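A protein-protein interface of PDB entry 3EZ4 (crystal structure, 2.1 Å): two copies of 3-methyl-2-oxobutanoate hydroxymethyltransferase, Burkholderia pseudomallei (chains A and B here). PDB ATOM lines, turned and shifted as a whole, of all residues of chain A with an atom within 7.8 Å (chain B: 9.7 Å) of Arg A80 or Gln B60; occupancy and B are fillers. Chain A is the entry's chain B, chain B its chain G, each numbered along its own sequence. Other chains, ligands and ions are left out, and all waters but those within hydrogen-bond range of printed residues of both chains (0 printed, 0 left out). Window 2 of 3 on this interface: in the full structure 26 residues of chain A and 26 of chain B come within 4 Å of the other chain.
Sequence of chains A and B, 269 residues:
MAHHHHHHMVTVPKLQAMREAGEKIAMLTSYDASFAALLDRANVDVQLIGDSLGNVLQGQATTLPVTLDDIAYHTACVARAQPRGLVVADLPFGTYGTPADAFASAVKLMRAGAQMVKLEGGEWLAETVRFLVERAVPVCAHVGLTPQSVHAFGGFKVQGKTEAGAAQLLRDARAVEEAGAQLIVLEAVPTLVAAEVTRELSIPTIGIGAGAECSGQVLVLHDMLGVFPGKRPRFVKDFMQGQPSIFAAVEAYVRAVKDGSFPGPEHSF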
ATOM      1  N   ASP A  32     -19.691  18.561 -17.364  1.00  0.00           N
ATOM      2  CA  ASP A  32     -20.232  18.114 -18.645  1.00  0.00           C
ATOM      3  C   ASP A  32     -19.349  17.140 -19.402  1.00  0.00           C
ATOM      4  O   ASP A  32     -18.212  16.929 -19.026  1.00  0.00           O
ATOM      5  CB  ASP A  32     -20.605  19.281 -19.557  1.00  0.00           C
ATOM      6  CG  ASP A  32     -19.388  20.104 -20.023  1.00  0.00           C
ATOM      7  OD1 ASP A  32     -18.653  19.643 -20.944  1.00  0.00           O
ATOM      8  OD2 ASP A  32     -19.233  21.235 -19.502  1.00  0.00           O
ATOM      9  N   ALA A  33     -19.938  16.521 -20.431  1.00  0.00           N
ATOM     10  CA  ALA A  33     -19.338  15.401 -21.159  1.00  0.00           C
ATOM     11  C   ALA A  33     -18.140  15.869 -22.001  1.00  0.00           C
ATOM     12  O   ALA A  33     -17.132  15.209 -22.011  1.00  0.00           O
ATOM     13  CB  ALA A  33     -20.380  14.693 -22.032  1.00  0.00           C
ATOM     14  N   ALA A  36     -15.373  16.681 -19.635  1.00  0.00           N
ATOM     15  CA  ALA A  36     -15.016  15.385 -19.020  1.00  0.00           C
ATOM     16  C   ALA A  36     -14.073  14.544 -19.926  1.00  0.00           C
ATOM     17  O   ALA A  36     -13.110  13.990 -19.418  1.00  0.00           O
ATOM     18  CB  ALA A  36     -16.244  14.577 -18.588  1.00  0.00           C
ATOM     19  N   ALA A  37     -14.353  14.478 -21.237  1.00  0.00           N
ATOM     20  CA  ALA A  37     -13.508  13.756 -22.207  1.00  0.00           C
ATOM     21  C   ALA A  37     -12.136  14.408 -22.360  1.00  0.00           C
ATOM     22  O   ALA A  37     -11.128  13.750 -22.366  1.00  0.00           O
ATOM     23  CB  ALA A  37     -14.208  13.603 -23.592  1.00  0.00           C
ATOM     24  N   ALA A  72     -27.003  15.574  -9.586  1.00  0.00           N
ATOM     25  CA  ALA A  72     -27.253  14.315 -10.334  1.00  0.00           C
ATOM     26  C   ALA A  72     -27.262  14.545 -11.870  1.00  0.00           C
ATOM     27  O   ALA A  72     -26.760  13.702 -12.661  1.00  0.00           O
ATOM     28  CB  ALA A  72     -28.555  13.665  -9.889  1.00  0.00           C
ATOM     29  N   TYR A  73     -27.813  15.680 -12.311  1.00  0.00           N
ATOM     30  CA  TYR A  73     -27.827  15.944 -13.764  1.00  0.00           C
ATOM     31  C   TYR A  73     -26.379  16.104 -14.269  1.00  0.00           C
ATOM     32  O   TYR A  73     -25.990  15.478 -15.237  1.00  0.00           O
ATOM     33  CB  TYR A  73     -28.661  17.191 -14.030  1.00  0.00           C
ATOM     34  CG  TYR A  73     -28.626  17.718 -15.456  1.00  0.00           C
ATOM     35  CD1 TYR A  73     -29.327  17.094 -16.467  1.00  0.00           C
ATOM     36  CD2 TYR A  73     -27.879  18.830 -15.762  1.00  0.00           C
ATOM     37  CE1 TYR A  73     -29.312  17.621 -17.783  1.00  0.00           C
ATOM     38  CE2 TYR A  73     -27.822  19.342 -17.069  1.00  0.00           C
ATOM     39  CZ  TYR A  73     -28.516  18.737 -18.066  1.00  0.00           C
ATOM     40  OH  TYR A  73     -28.462  19.263 -19.345  1.00  0.00           O
ATOM     41  N   HIS A  74     -25.563  16.904 -13.589  1.00  0.00           N
ATOM     42  CA  HIS A  74     -24.208  17.107 -14.036  1.00  0.00           C
ATOM     43  C   HIS A  74     -23.327  15.848 -13.865  1.00  0.00           C
ATOM     44  O   HIS A  74     -22.441  15.586 -14.661  1.00  0.00           O
ATOM     45  CB  HIS A  74     -23.628  18.342 -13.346  1.00  0.00           C
ATOM     46  CG  HIS A  74     -24.280  19.625 -13.789  1.00  0.00           C
ATOM     47  ND1 HIS A  74     -24.012  20.206 -15.012  1.00  0.00           N
ATOM     48  CD2 HIS A  74     -25.191  20.428 -13.176  1.00  0.00           C
ATOM     49  CE1 HIS A  74     -24.753  21.302 -15.149  1.00  0.00           C
ATOM     50  NE2 HIS A  74     -25.485  21.456 -14.046  1.00  0.00           N
ATOM     51  N   THR A  75     -23.575  15.056 -12.823  1.00  0.00           N
ATOM     52  CA  THR A  75     -22.909  13.791 -12.664  1.00  0.00           C
ATOM     53  C   THR A  75     -23.233  12.856 -13.851  1.00  0.00           C
ATOM     54  O   THR A  75     -22.357  12.281 -14.425  1.00  0.00           O
ATOM     55  CB  THR A  75     -23.347  13.110 -11.350  1.00  0.00           C
ATOM     56  OG1 THR A  75     -23.009  13.927 -10.231  1.00  0.00           O
ATOM     57  CG2 THR A  75     -22.673  11.718 -11.219  1.00  0.00           C
ATOM     58  N   ALA A  76     -24.497  12.719 -14.223  1.00  0.00           N
ATOM     59  CA  ALA A  76     -24.860  11.923 -15.396  1.00  0.00           C
ATOM     60  C   ALA A  76     -24.147  12.384 -16.723  1.00  0.00           C
ATOM     61  O   ALA A  76     -23.702  11.532 -17.535  1.00  0.00           O
ATOM     62  CB  ALA A  76     -26.388  11.855 -15.537  1.00  0.00           C
ATOM     63  N   CYS A  77     -24.055  13.697 -16.953  1.00  0.00           N
ATOM     64  CA  CYS A  77     -23.278  14.227 -18.073  1.00  0.00           C
ATOM     65  C   CYS A  77     -21.805  13.766 -18.104  1.00  0.00           C
ATOM     66  O   CYS A  77     -21.322  13.312 -19.160  1.00  0.00           O
ATOM     67  CB  CYS A  77     -23.298  15.753 -18.042  1.00  0.00           C
ATOM     68  SG  CYS A  77     -24.974  16.436 -18.355  1.00  0.00           S
ATOM     69  N   VAL A  78     -21.106  13.926 -16.969  1.00  0.00           N
ATOM     70  CA  VAL A  78     -19.704  13.518 -16.817  1.00  0.00           C
ATOM     71  C   VAL A  78     -19.546  12.018 -17.035  1.00  0.00           C
ATOM     72  O   VAL A  78     -18.684  11.571 -17.791  1.00  0.00           O
ATOM     73  CB  VAL A  78     -19.151  13.992 -15.464  1.00  0.00           C
ATOM     74  CG1 VAL A  78     -17.764  13.472 -15.162  1.00  0.00           C
ATOM     75  CG2 VAL A  78     -19.146  15.498 -15.414  1.00  0.00           C
ATOM     76  N   ALA A  79     -20.438  11.234 -16.442  1.00  0.00           N
ATOM     77  CA  ALA A  79     -20.296   9.783 -16.473  1.00  0.00           C
ATOM     78  C   ALA A  79     -20.511   9.299 -17.864  1.00  0.00           C
ATOM     79  O   ALA A  79     -19.965   8.274 -18.234  1.00  0.00           O
ATOM     80  CB  ALA A  79     -21.274   9.053 -15.497  1.00  0.00           C
ATOM     81  N   ARG A  80     -21.252  10.051 -18.666  1.00  0.00           N
ATOM     82  CA  ARG A  80     -21.566   9.585 -19.995  1.00  0.00           C
ATOM     83  C   ARG A  80     -20.352   9.678 -20.907  1.00  0.00           C
ATOM     84  O   ARG A  80     -20.289   8.966 -21.882  1.00  0.00           O
ATOM     85  CB  ARG A  80     -22.769  10.363 -20.536  1.00  0.00           C
ATOM     86  CG  ARG A  80     -23.384   9.737 -21.773  1.00  0.00           C
ATOM     87  CD  ARG A  80     -24.871   9.638 -21.596  1.00  0.00           C
ATOM     88  NE  ARG A  80     -25.367  10.898 -21.072  1.00  0.00           N
ATOM     89  CZ  ARG A  80     -26.388  11.050 -20.247  1.00  0.00           C
ATOM     90  NH1 ARG A  80     -27.093  10.001 -19.855  1.00  0.00           N
ATOM     91  NH2 ARG A  80     -26.689  12.280 -19.827  1.00  0.00           N
ATOM     92  N   ALA A  81     -19.371  10.525 -20.566  1.00  0.00           N
ATOM     93  CA  ALA A  81     -18.070  10.532 -21.232  1.00  0.00           C
ATOM     94  C   ALA A  81     -17.237   9.315 -20.912  1.00  0.00           C
ATOM     95  O   ALA A  81     -16.210   9.099 -21.521  1.00  0.00           O
ATOM     96  CB  ALA A  81     -17.263  11.794 -20.848  1.00  0.00           C
ATOM     97  N   GLN A  82     -17.646   8.533 -19.920  1.00  0.00           N
ATOM     98  CA  GLN A  82     -16.937   7.306 -19.570  1.00  0.00           C
ATOM     99  C   GLN A  82     -15.443   7.524 -19.271  1.00  0.00           C
ATOM    100  O   GLN A  82     -14.573   6.861 -19.832  1.00  0.00           O
ATOM    101  CB  GLN A  82     -17.138   6.263 -20.672  1.00  0.00           C
ATOM    102  CG  GLN A  82     -18.532   5.692 -20.696  1.00  0.00           C
ATOM    103  CD  GLN A  82     -18.502   4.295 -21.257  1.00  0.00           C
ATOM    104  OE1 GLN A  82     -18.135   4.112 -22.415  1.00  0.00           O
ATOM    105  NE2 GLN A  82     -18.800   3.286 -20.415  1.00  0.00           N
ATOM    106  N   PRO A  83     -15.151   8.416 -18.319  1.00  0.00           N
ATOM    107  CA  PRO A  83     -13.756   8.718 -18.054  1.00  0.00           C
ATOM    108  C   PRO A  83     -13.063   7.589 -17.312  1.00  0.00           C
ATOM    109  O   PRO A  83     -13.712   6.813 -16.639  1.00  0.00           O
ATOM    110  CB  PRO A  83     -13.817   9.987 -17.211  1.00  0.00           C
ATOM    111  CG  PRO A  83     -15.200  10.144 -16.757  1.00  0.00           C
ATOM    112  CD  PRO A  83     -16.080   9.200 -17.494  1.00  0.00           C
ATOM    113  N   VAL A  87     -14.941   9.522 -10.639  1.00  0.00           N
ATOM    114  CA  VAL A  87     -15.977  10.514 -10.620  1.00  0.00           C
ATOM    115  C   VAL A  87     -16.502  10.662  -9.193  1.00  0.00           C
ATOM    116  O   VAL A  87     -17.049   9.736  -8.597  1.00  0.00           O
ATOM    117  CB  VAL A  87     -17.134  10.121 -11.605  1.00  0.00           C
ATOM    118  CG1 VAL A  87     -18.253  11.123 -11.538  1.00  0.00           C
ATOM    119  CG2 VAL A  87     -16.606   9.997 -13.055  1.00  0.00           C
ATOM    120  N   ALA A 112     -26.614   7.784 -10.713  1.00  0.00           N
ATOM    121  CA  ALA A 112     -26.302   8.694 -11.856  1.00  0.00           C
ATOM    122  C   ALA A 112     -24.874   8.584 -12.376  1.00  0.00           C
ATOM    123  O   ALA A 112     -24.547   9.213 -13.368  1.00  0.00           O
ATOM    124  CB  ALA A 112     -26.592  10.179 -11.489  1.00  0.00           C
ATOM    125  N   GLY A 113     -24.011   7.841 -11.689  1.00  0.00           N
ATOM    126  CA  GLY A 113     -22.661   7.673 -12.149  1.00  0.00           C
ATOM    127  C   GLY A 113     -21.553   8.060 -11.203  1.00  0.00           C
ATOM    128  O   GLY A 113     -20.388   7.784 -11.506  1.00  0.00           O
ATOM    129  N   ASP B  51     -30.385  22.734 -28.608  1.00  0.00           N
ATOM    130  CA  ASP B  51     -30.395  21.307 -28.226  1.00  0.00           C
ATOM    131  C   ASP B  51     -29.125  20.546 -28.567  1.00  0.00           C
ATOM    132  O   ASP B  51     -28.948  19.388 -28.174  1.00  0.00           O
ATOM    133  CB  ASP B  51     -31.658  20.596 -28.692  1.00  0.00           C
ATOM    134  CG  ASP B  51     -31.763  20.496 -30.222  1.00  0.00           C
ATOM    135  OD1 ASP B  51     -30.843  20.930 -30.965  1.00  0.00           O
ATOM    136  OD2 ASP B  51     -32.811  19.948 -30.670  1.00  0.00           O
ATOM    137  N   SER B  52     -28.202  21.246 -29.228  1.00  0.00           N
ATOM    138  CA  SER B  52     -26.818  20.860 -29.278  1.00  0.00           C
ATOM    139  C   SER B  52     -26.258  20.479 -27.897  1.00  0.00           C
ATOM    140  O   SER B  52     -25.355  19.720 -27.848  1.00  0.00           O
ATOM    141  CB  SER B  52     -25.962  22.001 -29.918  1.00  0.00           C
ATOM    142  OG  SER B  52     -25.936  23.173 -29.113  1.00  0.00           O
ATOM    143  N   LEU B  53     -26.793  21.021 -26.788  1.00  0.00           N
ATOM    144  CA  LEU B  53     -26.339  20.652 -25.431  1.00  0.00           C
ATOM    145  C   LEU B  53     -26.510  19.136 -25.178  1.00  0.00           C
ATOM    146  O   LEU B  53     -25.771  18.563 -24.368  1.00  0.00           O
ATOM    147  CB  LEU B  53     -27.064  21.493 -24.341  1.00  0.00           C
ATOM    148  CG  LEU B  53     -28.553  21.235 -24.076  1.00  0.00           C
ATOM    149  CD1 LEU B  53     -28.803  20.046 -23.085  1.00  0.00           C
ATOM    150  CD2 LEU B  53     -29.247  22.555 -23.652  1.00  0.00           C
ATOM    151  N   GLY B  54     -27.406  18.488 -25.935  1.00  0.00           N
ATOM    152  CA  GLY B  54     -27.541  17.027 -25.899  1.00  0.00           C
ATOM    153  C   GLY B  54     -26.258  16.263 -26.233  1.00  0.00           C
ATOM    154  O   GLY B  54     -25.926  15.241 -25.572  1.00  0.00           O
ATOM    155  N   ASN B  55     -25.510  16.764 -27.228  1.00  0.00           N
ATOM    156  CA  ASN B  55     -24.208  16.220 -27.581  1.00  0.00           C
ATOM    157  C   ASN B  55     -23.130  16.811 -26.682  1.00  0.00           C
ATOM    158  O   ASN B  55     -22.457  16.075 -25.935  1.00  0.00           O
ATOM    159  CB  ASN B  55     -23.835  16.477 -29.058  1.00  0.00           C
ATOM    160  CG  ASN B  55     -24.903  16.001 -30.048  1.00  0.00           C
ATOM    161  OD1 ASN B  55     -25.447  16.788 -30.842  1.00  0.00           O
ATOM    162  ND2 ASN B  55     -25.236  14.724 -29.975  1.00  0.00           N
ATOM    163  N   VAL B  56     -22.995  18.136 -26.653  1.00  0.00           N
ATOM    164  CA  VAL B  56     -21.775  18.750 -26.073  1.00  0.00           C
ATOM    165  C   VAL B  56     -21.727  18.719 -24.530  1.00  0.00           C
ATOM    166  O   VAL B  56     -20.658  18.521 -23.938  1.00  0.00           O
ATOM    167  CB  VAL B  56     -21.517  20.189 -26.621  1.00  0.00           C
ATOM    168  CG1 VAL B  56     -21.487  20.149 -28.142  1.00  0.00           C
ATOM    169  CG2 VAL B  56     -22.563  21.168 -26.149  1.00  0.00           C
ATOM    170  N   LEU B  57     -22.874  18.863 -23.868  1.00  0.00           N
ATOM    171  CA  LEU B  57     -22.906  18.802 -22.406  1.00  0.00           C
ATOM    172  C   LEU B  57     -23.328  17.384 -21.919  1.00  0.00           C
ATOM    173  O   LEU B  57     -22.703  16.828 -21.009  1.00  0.00           O
ATOM    174  CB  LEU B  57     -23.845  19.860 -21.821  1.00  0.00           C
ATOM    175  CG  LEU B  57     -23.630  21.335 -22.136  1.00  0.00           C
ATOM    176  CD1 LEU B  57     -24.508  22.226 -21.215  1.00  0.00           C
ATOM    177  CD2 LEU B  57     -22.168  21.695 -22.010  1.00  0.00           C
ATOM    178  N   GLN B  58     -24.342  16.776 -22.562  1.00  0.00           N
ATOM    179  CA  GLN B  58     -24.914  15.546 -22.014  1.00  0.00           C
ATOM    180  C   GLN B  58     -24.212  14.301 -22.548  1.00  0.00           C
ATOM    181  O   GLN B  58     -24.428  13.188 -22.052  1.00  0.00           O
ATOM    182  CB  GLN B  58     -26.436  15.473 -22.244  1.00  0.00           C
ATOM    183  CG  GLN B  58     -27.218  16.525 -21.486  1.00  0.00           C
ATOM    184  CD  GLN B  58     -28.731  16.517 -21.771  1.00  0.00           C
ATOM    185  OE1 GLN B  58     -29.515  17.315 -21.189  1.00  0.00           O
ATOM    186  NE2 GLN B  58     -29.138  15.685 -22.681  1.00  0.00           N
ATOM    187  N   GLY B  59     -23.414  14.493 -23.590  1.00  0.00           N
ATOM    188  CA  GLY B  59     -22.686  13.406 -24.215  1.00  0.00           C
ATOM    189  C   GLY B  59     -23.523  12.355 -24.908  1.00  0.00           C
ATOM    190  O   GLY B  59     -23.089  11.222 -25.014  1.00  0.00           O
ATOM    191  N   GLN B  60     -24.703  12.718 -25.405  1.00  0.00           N
ATOM    192  CA  GLN B  60     -25.564  11.761 -26.124  1.00  0.00           C
ATOM    193  C   GLN B  60     -25.190  11.794 -27.603  1.00  0.00           C
ATOM    194  O   GLN B  60     -24.639  12.804 -28.100  1.00  0.00           O
ATOM    195  CB  GLN B  60     -27.028  12.168 -25.988  1.00  0.00           C
ATOM    196  CG  GLN B  60     -27.525  12.379 -24.572  1.00  0.00           C
ATOM    197  CD  GLN B  60     -28.030  11.101 -23.910  1.00  0.00           C
ATOM    198  OE1 GLN B  60     -27.695  10.013 -24.334  1.00  0.00           O
ATOM    199  NE2 GLN B  60     -28.847  11.244 -22.855  1.00  0.00           N
ATOM    200  N   ALA B  61     -25.551  10.741 -28.334  1.00  0.00           N
ATOM    201  CA  ALA B  61     -25.256  10.646 -29.800  1.00  0.00           C
ATOM    202  C   ALA B  61     -26.169  11.491 -30.643  1.00  0.00           C
ATOM    203  O   ALA B  61     -25.810  11.892 -31.738  1.00  0.00           O
ATOM    204  CB  ALA B  61     -25.315   9.153 -30.292  1.00  0.00           C
ATOM    205  N   THR B  62     -27.368  11.746 -30.164  1.00  0.00           N
ATOM    206  CA  THR B  62     -28.289  12.627 -30.850  1.00  0.00           C
ATOM    207  C   THR B  62     -28.874  13.601 -29.825  1.00  0.00           C
ATOM    208  O   THR B  62     -28.604  13.503 -28.614  1.00  0.00           O
ATOM    209  CB  THR B  62     -29.495  11.887 -31.542  1.00  0.00           C
ATOM    210  OG1 THR B  62     -30.452  11.538 -30.546  1.00  0.00           O
ATOM    211  CG2 THR B  62     -29.053  10.644 -32.387  1.00  0.00           C
ATOM    212  N   THR B  63     -29.684  14.531 -30.318  1.00  0.00           N
ATOM    213  CA  THR B  63     -30.263  15.584 -29.490  1.00  0.00           C
ATOM    214  C   THR B  63     -31.674  15.234 -29.003  1.00  0.00           C
ATOM    215  O   THR B  63     -32.278  15.954 -28.217  1.00  0.00           O
ATOM    216  CB  THR B  63     -30.300  16.847 -30.271  1.00  0.00           C
ATOM    217  OG1 THR B  63     -31.124  16.644 -31.407  1.00  0.00           O
ATOM    218  CG2 THR B  63     -28.882  17.246 -30.781  1.00  0.00           C
ATOM    219  N   LEU B  64     -32.192  14.091 -29.434  1.00  0.00           N
ATOM    220  CA  LEU B  64     -33.563  13.720 -29.142  1.00  0.00           C
ATOM    221  C   LEU B  64     -33.845  13.558 -27.658  1.00  0.00           C
ATOM    222  O   LEU B  64     -34.952  13.832 -27.245  1.00  0.00           O
ATOM    223  CB  LEU B  64     -33.977  12.438 -29.898  1.00  0.00           C
ATOM    224  CG  LEU B  64     -34.105  12.556 -31.443  1.00  0.00           C
ATOM    225  CD1 LEU B  64     -34.687  11.271 -32.052  1.00  0.00           C
ATOM    226  CD2 LEU B  64     -35.058  13.618 -31.735  1.00  0.00           C
ATOM    227  N   PRO B  65     -32.855  13.148 -26.859  1.00  0.00           N
ATOM    228  CA  PRO B  65     -33.176  13.023 -25.411  1.00  0.00           C
ATOM    229  C   PRO B  65     -33.291  14.352 -24.645  1.00  0.00           C
ATOM    230  O   PRO B  65     -33.723  14.344 -23.497  1.00  0.00           O
ATOM    231  CB  PRO B  65     -32.014  12.190 -24.852  1.00  0.00           C
ATOM    232  CG  PRO B  65     -31.363  11.475 -26.095  1.00  0.00           C
ATOM    233  CD  PRO B  65     -31.582  12.482 -27.228  1.00  0.00           C
ATOM    234  N   VAL B  66     -32.930  15.471 -25.267  1.00  0.00           N
ATOM    235  CA  VAL B  66     -32.966  16.784 -24.605  1.00  0.00           C
ATOM    236  C   VAL B  66     -34.417  17.192 -24.307  1.00  0.00           C
ATOM    237  O   VAL B  66     -35.262  17.168 -25.195  1.00  0.00           O
ATOM    238  CB  VAL B  66     -32.243  17.867 -25.477  1.00  0.00           C
ATOM    239  CG1 VAL B  66     -32.386  19.258 -24.862  1.00  0.00           C
ATOM    240  CG2 VAL B  66     -30.759  17.522 -25.633  1.00  0.00           C
ATOM    241  N   THR B  67     -34.707  17.532 -23.051  1.00  0.00           N
ATOM    242  CA  THR B  67     -36.058  17.833 -22.671  1.00  0.00           C
ATOM    243  C   THR B  67     -36.230  19.324 -22.571  1.00  0.00           C
ATOM    244  O   THR B  67     -35.269  20.047 -22.587  1.00  0.00           O
ATOM    245  CB  THR B  67     -36.456  17.246 -21.283  1.00  0.00           C
ATOM    246  OG1 THR B  67     -35.653  17.863 -20.281  1.00  0.00           O
ATOM    247  CG2 THR B  67     -36.238  15.688 -21.209  1.00  0.00           C
ATOM    248  N   ASP B  70     -34.525  20.620 -19.459  1.00  0.00           N
ATOM    249  CA  ASP B  70     -33.082  20.812 -19.699  1.00  0.00           C
ATOM    250  C   ASP B  70     -32.833  22.199 -20.289  1.00  0.00           C
ATOM    251  O   ASP B  70     -31.960  22.924 -19.820  1.00  0.00           O
ATOM    252  CB  ASP B  70     -32.538  19.786 -20.706  1.00  0.00           C
ATOM    253  CG  ASP B  70     -32.556  18.357 -20.183  1.00  0.00           C
ATOM    254  OD1 ASP B  70     -32.554  18.202 -18.941  1.00  0.00           O
ATOM    255  OD2 ASP B  70     -32.507  17.407 -21.007  1.00  0.00           O
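The side-chain hydroxyl (OH) of Tyr A73 sits at hydrogen-bond distance from the side-chain amide oxygen (OE1) of Gln B58, 2.9 Å away. The backbone carbonyl oxygen (O) of Leu B57 is in hydrogen-bond range of the backbone NH (N) of Ala A33. The backbone carbonyl oxygen (O) of Leu B57 sits close to the side-chain sulfur (SG) of Cys A77. The guanidinium group (NE) of Arg A80 sits at hydrogen-bond distance from the backbone carbonyl oxygen (O) of Gln B58 (2.7 Å).
The side-chain carboxylate of Asp B70 sits close to the side-chain amide oxygen of Gln B58, 3.0 Å away. The backbone carbonyl oxygen (O) of Gly B54 sits at hydrogen-bond distance from the backbone NH (N) of Gln B60 (2.8 Å). The side-chain sulfur (SG) of Cys A77 lies within hydrogen-bond range of the backbone carbonyl oxygen (O) of Tyr A73 (3.4 Å). The backbone NH (N) of Thr B67 lies within hydrogen-bond range of the side-chain carboxylate (OD2) of Asp B70 (3.0 Å). The backbone carbonyl oxygen (O) of Gly B54 lies within hydrogen-bond range of the backbone NH (N) of Gly B59 (3.3 Å). The backbone carbonyl oxygen (O) of Leu B53 lies within hydrogen-bond range of the backbone NH (N) of Gln B58 (2.9 Å).
Val B56 touches Asp A32. Asp A32 touches Leu B57 (CB to O, 3.5 Å). C of Gln B58 touches CB of Ala A33, 3.9 Å away. CB of Ala A33 touches N of Gly B59 (3.4 Å). Leu B53 touches Tyr A73 (CD1 to OH, 3.8 Å). Asp B70 touches Tyr A73. Gln B58 touches Cys A77 (CA to SG, 3.8 Å). Arg A80 touches Gly B59 (CG to O, 3.6 Å). Arg A80 touches Gln B60.
Of the printed residues of chain B, Ala A33 touches Leu B57, Gln B58 and Gly B59. Of chain B, only Leu B57 (3.2 Å) and Gln B58 (3.8 Å) come within 4 Å of Cys A77. No residue of chain B comes within 4 Å of Ala A79. Of chain B, only Gln B58, Gly B59 and Gln B60 come within 4 Å of Arg A80. No residue of chain B comes within 4 Å of Ala A81. Printed residues of chain A within 4 Å of Gln B58: Ala A33, Tyr A73, Cys A77 and Arg A80. Gly B59 touches two residues of chain A. Of chain A, only Arg A80 comes within 4 Å of Gln B60. Of the printed residues of chain A, Asp B70 touches Tyr A73. The nearest residue of chain A that does not touch Gln B60 is Ala A33 (5.8 Å). The nearest printed residue of chain A that does not touch Leu B53 is Cys A77 (6.4 Å).
Of the 19 printed residues of chain A, 5 touch a printed residue of chain B. Among the printed residues, no Asp or Glu carboxylate lies within 4 Å of a Lys or Arg side-chain nitrogen of the other chain.
No position is printed for both chains. Of the 13 pairs that touch across the chains among the printed residues, none has its exchanged pair printed and touching as well.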
